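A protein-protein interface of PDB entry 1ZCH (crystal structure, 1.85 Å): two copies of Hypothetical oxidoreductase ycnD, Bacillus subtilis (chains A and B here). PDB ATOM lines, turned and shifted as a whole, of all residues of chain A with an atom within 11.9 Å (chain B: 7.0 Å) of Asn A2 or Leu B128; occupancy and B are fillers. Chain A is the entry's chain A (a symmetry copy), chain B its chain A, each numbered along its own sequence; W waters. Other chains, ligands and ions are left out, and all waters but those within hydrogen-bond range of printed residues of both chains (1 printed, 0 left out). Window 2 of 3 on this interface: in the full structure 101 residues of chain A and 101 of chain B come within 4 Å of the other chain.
The side-chain hydroxyl (OG) of Ser B127 lies within hydrogen-bond range of the side-chain amide nitrogen (ND2) of Asn A2, at 3.2 Å.
The backbone carbonyl oxygen (O) of Glu B25 sits close to the side-chain amide nitrogen (NE2) of Gln B29 (3.5 Å). OG of Ser B127 sits at hydrogen-bond distance from O of Ala B124 (2.6 Å). OD1 of Asn A2 is in hydrogen-bond range of N of Val A4 (2.9 Å). The backbone NH of Ile A5 lies within hydrogen-bond range of the side-chain amide oxygen of Asn A2 (2.7 Å). The side-chain hydroxyl (OG1) of Thr A9 lies within hydrogen-bond range of the backbone carbonyl oxygen (O) of Ile A5, 2.8 Å away.
Asn A2 touches Leu B128. Ser B127 touches Val A4. Ile A5 touches Gln B29. Ile A5 touches Ala B124 (CD1 to CB, 3.6 Å). OG of Ser B127 touches CD1 of Ile A5, at 3.7 Å. Ala B124 touches Leu A8 (CB to CD1, 3.9 Å).
Printed residues of chain B within 4 Å of Asn A2: Ser B127 and Leu B128. Leu B128 touches one residue of chain A. No residue of chain A comes within 4 Å of Gln B26. Gln B29 touches one residue of chain A. Of chain A, only Ile A5 and Leu A8 come within 4 Å of Ala B124. No residue of chain A comes within 4 Å of Ala B125. Of chain A, only Asn A2 (3.2 Å), Val A4 (3.4 Å) and Ile A5 (3.7 Å) come within 4 Å of Ser B127. No residue of chain A comes within 4 Å of Gly B129. Of the printed residues of chain B, Ile A5 touches Gln B29 (3.9 Å), Ala B124 (3.6 Å) and Ser B127 (3.7 Å). Printed residues of chain B within 4 Å of Val A4: Ser B127. Ser A127 touches none of the printed residues of chain B. The nearest residue of chain B that does not touch Asn A2 is Gln B29 (4.9 Å). The nearest residue of chain A that does not touch Leu B128 is Ile A5 (4.3 Å). The nearest printed residue of chain B that does not touch Leu A8 is Ala B123 (4.5 Å).
Printed residues of chain A that touch a printed residue of chain B: Asn A2, Val A4, Ile A5 and Leu A8. Hydrophobic or aromatic side chains of chain A that line the printed part of chain B: Val A4, Ile A5 and Leu A8. Of the 18 printed residues of chain B, 4 touch a printed residue of chain A. Printed residues of chain B that touch a printed residue of chain A: Gln B29, Ala B124, Ser B127 and Leu B128. Among the printed residues, no Asp or Glu carboxylate lies within 4 Å of a Lys or Arg side-chain nitrogen of the other chain.
Positions printed for both chains: 7, 123 and 127.
Water W1 bridges the side-chain amide oxygen (OE1) of Gln B29 and the backbone NH (N) of Asn A2.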
ATOM      1  N   MET A   1      30.067 -23.740 -36.252  1.00  0.00           N
ATOM      2  CA  MET A   1      29.162 -23.529 -35.086  1.00  0.00           C
ATOM      3  C   MET A   1      27.930 -24.422 -35.213  1.00  0.00           C
ATOM      4  O   MET A   1      27.188 -24.332 -36.192  1.00  0.00           O
ATOM      5  CB  MET A   1      28.743 -22.057 -35.019  1.00  0.00           C
ATOM      6  CG  MET A   1      27.941 -21.684 -33.787  1.00  0.00           C
ATOM      7  SD  MET A   1      27.590 -19.914 -33.701  1.00  0.00           S
ATOM      8  CE  MET A   1      29.067 -19.309 -32.881  1.00  0.00           C
ATOM      9  N   ASN A   2      27.716 -25.285 -34.223  1.00  0.00           N
ATOM     10  CA  ASN A   2      26.575 -26.191 -34.243  1.00  0.00           C
ATOM     11  C   ASN A   2      25.271 -25.471 -33.916  1.00  0.00           C
ATOM     12  O   ASN A   2      25.272 -24.289 -33.567  1.00  0.00           O
ATOM     13  CB  ASN A   2      26.786 -27.351 -33.261  1.00  0.00           C
ATOM     14  CG  ASN A   2      26.896 -26.889 -31.820  1.00  0.00           C
ATOM     15  OD1 ASN A   2      26.123 -26.046 -31.367  1.00  0.00           O
ATOM     16  ND2 ASN A   2      27.849 -27.456 -31.087  1.00  0.00           N
ATOM     17  N   GLU A   3      24.163 -26.199 -34.025  1.00  0.00           N
ATOM     18  CA  GLU A   3      22.837 -25.646 -33.770  1.00  0.00           C
ATOM     19  C   GLU A   3      22.649 -25.097 -32.362  1.00  0.00           C
ATOM     20  O   GLU A   3      21.972 -24.089 -32.172  1.00  0.00           O
ATOM     21  CB  GLU A   3      21.768 -26.708 -34.048  1.00  0.00           C
ATOM     22  CG  GLU A   3      21.789 -27.231 -35.477  1.00  0.00           C
ATOM     23  CD  GLU A   3      21.535 -26.140 -36.503  1.00  0.00           C
ATOM     24  OE1 GLU A   3      21.827 -26.368 -37.695  1.00  0.00           O
ATOM     25  OE2 GLU A   3      21.039 -25.057 -36.122  1.00  0.00           O
ATOM     26  N   VAL A   4      23.237 -25.761 -31.373  1.00  0.00           N
ATOM     27  CA  VAL A   4      23.107 -25.304 -29.996  1.00  0.00           C
ATOM     28  C   VAL A   4      23.791 -23.955 -29.806  1.00  0.00           C
ATOM     29  O   VAL A   4      23.190 -23.020 -29.289  1.00  0.00           O
ATOM     30  CB  VAL A   4      23.714 -26.320 -29.009  1.00  0.00           C
ATOM     31  CG1 VAL A   4      23.614 -25.792 -27.587  1.00  0.00           C
ATOM     32  CG2 VAL A   4      22.981 -27.652 -29.128  1.00  0.00           C
ATOM     33  N   ILE A   5      25.048 -23.856 -30.229  1.00  0.00           N
ATOM     34  CA  ILE A   5      25.794 -22.611 -30.092  1.00  0.00           C
ATOM     35  C   ILE A   5      25.119 -21.502 -30.891  1.00  0.00           C
ATOM     36  O   ILE A   5      25.038 -20.360 -30.442  1.00  0.00           O
ATOM     37  CB  ILE A   5      27.251 -22.766 -30.582  1.00  0.00           C
ATOM     38  CG1 ILE A   5      27.953 -23.882 -29.806  1.00  0.00           C
ATOM     39  CG2 ILE A   5      28.003 -21.457 -30.393  1.00  0.00           C
ATOM     40  CD1 ILE A   5      28.090 -23.618 -28.321  1.00  0.00           C
ATOM     41  N   LYS A   6      24.634 -21.837 -32.083  1.00  0.00           N
ATOM     42  CA  LYS A   6      23.959 -20.840 -32.905  1.00  0.00           C
ATOM     43  C   LYS A   6      22.725 -20.303 -32.191  1.00  0.00           C
ATOM     44  O   LYS A   6      22.472 -19.101 -32.195  1.00  0.00           O
ATOM     45  CB  LYS A   6      23.540 -21.437 -34.252  1.00  0.00           C
ATOM     46  CG  LYS A   6      24.681 -21.634 -35.231  1.00  0.00           C
ATOM     47  CD  LYS A   6      24.149 -22.061 -36.594  1.00  0.00           C
ATOM     48  CE  LYS A   6      25.278 -22.242 -37.598  1.00  0.00           C
ATOM     49  NZ  LYS A   6      24.765 -22.703 -38.916  1.00  0.00           N
ATOM     50  N   SER A   7      21.956 -21.193 -31.573  1.00  0.00           N
ATOM     51  CA  SER A   7      20.750 -20.771 -30.877  1.00  0.00           C
ATOM     52  C   SER A   7      21.087 -19.915 -29.656  1.00  0.00           C
ATOM     53  O   SER A   7      20.483 -18.861 -29.449  1.00  0.00           O
ATOM     54  CB  SER A   7      19.921 -21.991 -30.456  1.00  0.00           C
ATOM     55  OG  SER A   7      18.643 -21.603 -29.973  1.00  0.00           O
ATOM     56  N   LEU A   8      22.058 -20.355 -28.859  1.00  0.00           N
ATOM     57  CA  LEU A   8      22.453 -19.612 -27.661  1.00  0.00           C
ATOM     58  C   LEU A   8      22.982 -18.212 -27.961  1.00  0.00           C
ATOM     59  O   LEU A   8      22.648 -17.250 -27.262  1.00  0.00           O
ATOM     60  CB  LEU A   8      23.520 -20.388 -26.877  1.00  0.00           C
ATOM     61  CG  LEU A   8      23.057 -21.708 -26.255  1.00  0.00           C
ATOM     62  CD1 LEU A   8      24.244 -22.420 -25.614  1.00  0.00           C
ATOM     63  CD2 LEU A   8      21.974 -21.433 -25.225  1.00  0.00           C
ATOM     64  N   THR A   9      23.805 -18.096 -28.996  1.00  0.00           N
ATOM     65  CA  THR A   9      24.386 -16.809 -29.351  1.00  0.00           C
ATOM     66  C   THR A   9      23.452 -15.873 -30.118  1.00  0.00           C
ATOM     67  O   THR A   9      23.811 -14.730 -30.390  1.00  0.00           O
ATOM     68  CB  THR A   9      25.706 -16.995 -30.145  1.00  0.00           C
ATOM     69  OG1 THR A   9      25.456 -17.732 -31.348  1.00  0.00           O
ATOM     70  CG2 THR A   9      26.719 -17.763 -29.304  1.00  0.00           C
ATOM     71  N   ASP A  10      22.254 -16.345 -30.454  1.00  0.00           N
ATOM     72  CA  ASP A  10      21.294 -15.508 -31.173  1.00  0.00           C
ATOM     73  C   ASP A  10      20.232 -14.951 -30.219  1.00  0.00           C
ATOM     74  O   ASP A  10      19.265 -14.318 -30.645  1.00  0.00           O
ATOM     75  CB  ASP A  10      20.612 -16.318 -32.281  1.00  0.00           C
ATOM     76  CG  ASP A  10      19.880 -15.436 -33.279  1.00  0.00           C
ATOM     77  OD1 ASP A  10      20.495 -14.466 -33.773  1.00  0.00           O
ATOM     78  OD2 ASP A  10      18.698 -15.713 -33.576  1.00  0.00           O
ATOM     79  N   HIS A  11      20.425 -15.181 -28.924  1.00  0.00           N
ATOM     80  CA  HIS A  11      19.472 -14.721 -27.920  1.00  0.00           C
ATOM     81  C   HIS A  11      19.197 -13.220 -27.837  1.00  0.00           C
ATOM     82  O   HIS A  11      20.097 -12.395 -27.985  1.00  0.00           O
ATOM     83  CB  HIS A  11      19.901 -15.169 -26.518  1.00  0.00           C
ATOM     84  CG  HIS A  11      19.142 -14.481 -25.424  1.00  0.00           C
ATOM     85  ND1 HIS A  11      17.865 -14.852 -25.060  1.00  0.00           N
ATOM     86  CD2 HIS A  11      19.431 -13.372 -24.702  1.00  0.00           C
ATOM     87  CE1 HIS A  11      17.398 -13.998 -24.165  1.00  0.00           C
ATOM     88  NE2 HIS A  11      18.327 -13.090 -23.931  1.00  0.00           N
ATOM     89  N   ALA A 123      17.115 -21.214 -22.993  1.00  0.00           N
ATOM     90  CA  ALA A 123      17.757 -21.857 -24.133  1.00  0.00           C
ATOM     91  C   ALA A 123      16.804 -22.821 -24.842  1.00  0.00           C
ATOM     92  O   ALA A 123      16.701 -22.825 -26.071  1.00  0.00           O
ATOM     93  CB  ALA A 123      19.002 -22.600 -23.671  1.00  0.00           C
ATOM     94  N   SER A 127      14.924 -22.278 -28.632  1.00  0.00           N
ATOM     95  CA  SER A 127      15.290 -23.231 -29.680  1.00  0.00           C
ATOM     96  C   SER A 127      14.021 -23.715 -30.393  1.00  0.00           C
ATOM     97  O   SER A 127      14.075 -24.206 -31.521  1.00  0.00           O
ATOM     98  CB  SER A 127      16.036 -24.437 -29.094  1.00  0.00           C
ATOM     99  OG  SER A 127      15.153 -25.347 -28.452  1.00  0.00           O
ATOM    100  N   SER B   7      20.261 -32.201 -26.833  1.00  0.00           N
ATOM    101  CA  SER B   7      21.509 -32.017 -26.108  1.00  0.00           C
ATOM    102  C   SER B   7      21.251 -31.723 -24.629  1.00  0.00           C
ATOM    103  O   SER B   7      21.888 -32.317 -23.756  1.00  0.00           O
ATOM    104  CB  SER B   7      22.332 -30.885 -26.737  1.00  0.00           C
ATOM    105  OG  SER B   7      23.641 -30.834 -26.186  1.00  0.00           O
ATOM    106  N   GLU B  25      39.236 -22.141 -29.586  1.00  0.00           N
ATOM    107  CA  GLU B  25      38.051 -21.806 -30.362  1.00  0.00           C
ATOM    108  C   GLU B  25      36.780 -22.285 -29.675  1.00  0.00           C
ATOM    109  O   GLU B  25      35.757 -21.601 -29.715  1.00  0.00           O
ATOM    110  CB  GLU B  25      38.134 -22.423 -31.758  1.00  0.00           C
ATOM    111  CG  GLU B  25      37.118 -21.853 -32.733  1.00  0.00           C
ATOM    112  CD  GLU B  25      37.238 -22.457 -34.120  1.00  0.00           C
ATOM    113  OE1 GLU B  25      38.369 -22.792 -34.527  1.00  0.00           O
ATOM    114  OE2 GLU B  25      36.203 -22.581 -34.809  1.00  0.00           O
ATOM    115  N   GLN B  26      36.840 -23.460 -29.054  1.00  0.00           N
ATOM    116  CA  GLN B  26      35.671 -23.996 -28.365  1.00  0.00           C
ATOM    117  C   GLN B  26      35.392 -23.171 -27.114  1.00  0.00           C
ATOM    118  O   GLN B  26      34.238 -22.876 -26.803  1.00  0.00           O
ATOM    119  CB  GLN B  26      35.883 -25.471 -28.003  1.00  0.00           C
ATOM    120  CG  GLN B  26      36.026 -26.381 -29.224  1.00  0.00           C
ATOM    121  CD  GLN B  26      36.075 -27.854 -28.857  1.00  0.00           C
ATOM    122  OE1 GLN B  26      36.818 -28.260 -27.966  1.00  0.00           O
ATOM    123  NE2 GLN B  26      35.285 -28.662 -29.551  1.00  0.00           N
ATOM    124  N   LEU B  27      36.448 -22.796 -26.397  1.00  0.00           N
ATOM    125  CA  LEU B  27      36.280 -21.980 -25.206  1.00  0.00           C
ATOM    126  C   LEU B  27      35.650 -20.644 -25.596  1.00  0.00           C
ATOM    127  O   LEU B  27      34.797 -20.121 -24.878  1.00  0.00           O
ATOM    128  CB  LEU B  27      37.630 -21.753 -24.515  1.00  0.00           C
ATOM    129  CG  LEU B  27      38.239 -22.983 -23.831  1.00  0.00           C
ATOM    130  CD1 LEU B  27      39.583 -22.623 -23.201  1.00  0.00           C
ATOM    131  CD2 LEU B  27      37.277 -23.501 -22.768  1.00  0.00           C
ATOM    132  N   GLN B  29      33.586 -20.064 -28.042  1.00  0.00           N
ATOM    133  CA  GLN B  29      32.172 -20.295 -28.325  1.00  0.00           C
ATOM    134  C   GLN B  29      31.371 -20.422 -27.033  1.00  0.00           C
ATOM    135  O   GLN B  29      30.264 -19.898 -26.924  1.00  0.00           O
ATOM    136  CB  GLN B  29      32.000 -21.562 -29.165  1.00  0.00           C
ATOM    137  CG  GLN B  29      32.545 -21.442 -30.577  1.00  0.00           C
ATOM    138  CD  GLN B  29      32.406 -22.730 -31.362  1.00  0.00           C
ATOM    139  OE1 GLN B  29      31.299 -23.208 -31.607  1.00  0.00           O
ATOM    140  NE2 GLN B  29      33.534 -23.301 -31.758  1.00  0.00           N
ATOM    141  N   ILE B  30      31.936 -21.132 -26.064  1.00  0.00           N
ATOM    142  CA  ILE B  30      31.283 -21.322 -24.776  1.00  0.00           C
ATOM    143  C   ILE B  30      31.107 -19.959 -24.103  1.00  0.00           C
ATOM    144  O   ILE B  30      30.041 -19.649 -23.571  1.00  0.00           O
ATOM    145  CB  ILE B  30      32.126 -22.261 -23.881  1.00  0.00           C
ATOM    146  CG1 ILE B  30      32.127 -23.672 -24.487  1.00  0.00           C
ATOM    147  CG2 ILE B  30      31.590 -22.263 -22.448  1.00  0.00           C
ATOM    148  CD1 ILE B  30      33.100 -24.626 -23.827  1.00  0.00           C
ATOM    149  N   THR B 122      27.395 -24.827 -19.507  1.00  0.00           N
ATOM    150  CA  THR B 122      27.259 -26.276 -19.475  1.00  0.00           C
ATOM    151  C   THR B 122      26.615 -26.752 -20.772  1.00  0.00           C
ATOM    152  O   THR B 122      27.099 -27.681 -21.414  1.00  0.00           O
ATOM    153  CB  THR B 122      26.390 -26.721 -18.278  1.00  0.00           C
ATOM    154  OG1 THR B 122      27.082 -26.427 -17.058  1.00  0.00           O
ATOM    155  CG2 THR B 122      26.100 -28.219 -18.345  1.00  0.00           C
ATOM    156  N   ALA B 123      25.522 -26.105 -21.156  1.00  0.00           N
ATOM    157  CA  ALA B 123      24.811 -26.467 -22.376  1.00  0.00           C
ATOM    158  C   ALA B 123      25.706 -26.331 -23.609  1.00  0.00           C
ATOM    159  O   ALA B 123      25.748 -27.216 -24.466  1.00  0.00           O
ATOM    160  CB  ALA B 123      23.575 -25.593 -22.530  1.00  0.00           C
ATOM    161  N   ALA B 124      26.427 -25.219 -23.690  1.00  0.00           N
ATOM    162  CA  ALA B 124      27.315 -24.966 -24.822  1.00  0.00           C
ATOM    163  C   ALA B 124      28.448 -25.985 -24.920  1.00  0.00           C
ATOM    164  O   ALA B 124      28.672 -26.587 -25.976  1.00  0.00           O
ATOM    165  CB  ALA B 124      27.899 -23.552 -24.719  1.00  0.00           C
ATOM    166  N   ALA B 125      29.158 -26.176 -23.814  1.00  0.00           N
ATOM    167  CA  ALA B 125      30.283 -27.104 -23.775  1.00  0.00           C
ATOM    168  C   ALA B 125      29.879 -28.523 -24.159  1.00  0.00           C
ATOM    169  O   ALA B 125      30.538 -29.171 -24.976  1.00  0.00           O
ATOM    170  CB  ALA B 125      30.908 -27.102 -22.379  1.00  0.00           C
ATOM    171  N   GLU B 126      28.794 -29.011 -23.570  1.00  0.00           N
ATOM    172  CA  GLU B 126      28.354 -30.367 -23.860  1.00  0.00           C
ATOM    173  C   GLU B 126      27.890 -30.548 -25.303  1.00  0.00           C
ATOM    174  O   GLU B 126      28.004 -31.644 -25.855  1.00  0.00           O
ATOM    175  CB  GLU B 126      27.282 -30.780 -22.841  1.00  0.00           C
ATOM    176  CG  GLU B 126      27.870 -30.774 -21.431  1.00  0.00           C
ATOM    177  CD  GLU B 126      26.912 -31.185 -20.330  1.00  0.00           C
ATOM    178  OE1 GLU B 126      25.709 -31.385 -20.595  1.00  0.00           O
ATOM    179  OE2 GLU B 126      27.383 -31.301 -19.181  1.00  0.00           O
ATOM    180  N   SER B 127      27.406 -29.478 -25.931  1.00  0.00           N
ATOM    181  CA  SER B 127      26.969 -29.566 -27.325  1.00  0.00           C
ATOM    182  C   SER B 127      28.190 -29.771 -28.229  1.00  0.00           C
ATOM    183  O   SER B 127      28.070 -30.243 -29.360  1.00  0.00           O
ATOM    184  CB  SER B 127      26.227 -28.292 -27.751  1.00  0.00           C
ATOM    185  OG  SER B 127      27.122 -27.217 -28.007  1.00  0.00           O
ATOM    186  N   LEU B 128      29.364 -29.415 -27.718  1.00  0.00           N
ATOM    187  CA  LEU B 128      30.607 -29.561 -28.467  1.00  0.00           C
ATOM    188  C   LEU B 128      31.255 -30.931 -28.248  1.00  0.00           C
ATOM    189  O   LEU B 128      32.305 -31.228 -28.821  1.00  0.00           O
ATOM    190  CB  LEU B 128      31.583 -28.453 -28.066  1.00  0.00           C
ATOM    191  CG  LEU B 128      31.120 -27.026 -28.393  1.00  0.00           C
ATOM    192  CD1 LEU B 128      32.024 -26.016 -27.707  1.00  0.00           C
ATOM    193  CD2 LEU B 128      31.125 -26.815 -29.903  1.00  0.00           C
ATOM    194  N   GLY B 129      30.630 -31.759 -27.420  1.00  0.00           N
ATOM    195  CA  GLY B 129      31.168 -33.081 -27.149  1.00  0.00           C
ATOM    196  C   GLY B 129      32.037 -33.107 -25.906  1.00  0.00           C
ATOM    197  O   GLY B 129      32.629 -34.135 -25.568  1.00  0.00           O
ATOM    198  N   LEU B 130      32.110 -31.976 -25.215  1.00  0.00           N
ATOM    199  CA  LEU B 130      32.916 -31.874 -24.004  1.00  0.00           C
ATOM    200  C   LEU B 130      32.144 -32.319 -22.770  1.00  0.00           C
ATOM    201  O   LEU B 130      30.915 -32.265 -22.735  1.00  0.00           O
ATOM    202  CB  LEU B 130      33.391 -30.430 -23.809  1.00  0.00           C
ATOM    203  CG  LEU B 130      34.289 -29.872 -24.917  1.00  0.00           C
ATOM    204  CD1 LEU B 130      34.382 -28.367 -24.792  1.00  0.00           C
ATOM    205  CD2 LEU B 130      35.669 -30.521 -24.832  1.00  0.00           C
ATOM    206  N   GLY B 131      32.880 -32.766 -21.759  1.00  0.00           N
ATOM    207  CA  GLY B 131      32.252 -33.184 -20.521  1.00  0.00           C
ATOM    208  C   GLY B 131      32.431 -32.057 -19.528  1.00  0.00           C
ATOM    209  O   GLY B 131      33.376 -31.273 -19.650  1.00  0.00           O
ATOM    210  N   HIS B 165      37.728 -33.320 -22.249  1.00  0.00           N
ATOM    211  CA  HIS B 165      37.249 -34.424 -23.068  1.00  0.00           C
ATOM    212  C   HIS B 165      36.996 -35.625 -22.155  1.00  0.00           C
ATOM    213  O   HIS B 165      37.865 -36.033 -21.387  1.00  0.00           O
ATOM    214  CB  HIS B 165      38.284 -34.738 -24.157  1.00  0.00           C
ATOM    215  CG  HIS B 165      38.436 -33.633 -25.159  1.00  0.00           C
ATOM    216  ND1 HIS B 165      37.536 -33.433 -26.182  1.00  0.00           N
ATOM    217  CD2 HIS B 165      39.337 -32.627 -25.250  1.00  0.00           C
ATOM    218  CE1 HIS B 165      37.874 -32.350 -26.861  1.00  0.00           C
ATOM    219  NE2 HIS B 165      38.964 -31.842 -26.315  1.00  0.00           N
ATOM    220  N   ARG B 169      31.920 -41.507 -20.361  1.00  0.00           N
ATOM    221  CA  ARG B 169      30.735 -40.664 -20.474  1.00  0.00           C
ATOM    222  C   ARG B 169      29.643 -40.930 -19.442  1.00  0.00           C
ATOM    223  O   ARG B 169      28.584 -40.305 -19.477  1.00  0.00           O
ATOM    224  CB  ARG B 169      30.170 -40.721 -21.898  1.00  0.00           C
ATOM    225  CG  ARG B 169      30.968 -39.859 -22.875  1.00  0.00           C
ATOM    226  CD  ARG B 169      30.317 -39.767 -24.246  1.00  0.00           C
ATOM    227  NE  ARG B 169      31.117 -38.979 -25.185  1.00  0.00           N
ATOM    228  CZ  ARG B 169      31.227 -37.652 -25.160  1.00  0.00           C
ATOM    229  NH1 ARG B 169      30.585 -36.944 -24.243  1.00  0.00           N
ATOM    230  NH2 ARG B 169      31.982 -37.031 -26.060  1.00  0.00           N
HETATM  231  O   HOH W   1      29.895 -25.190 -32.639  1.00  0.00           O
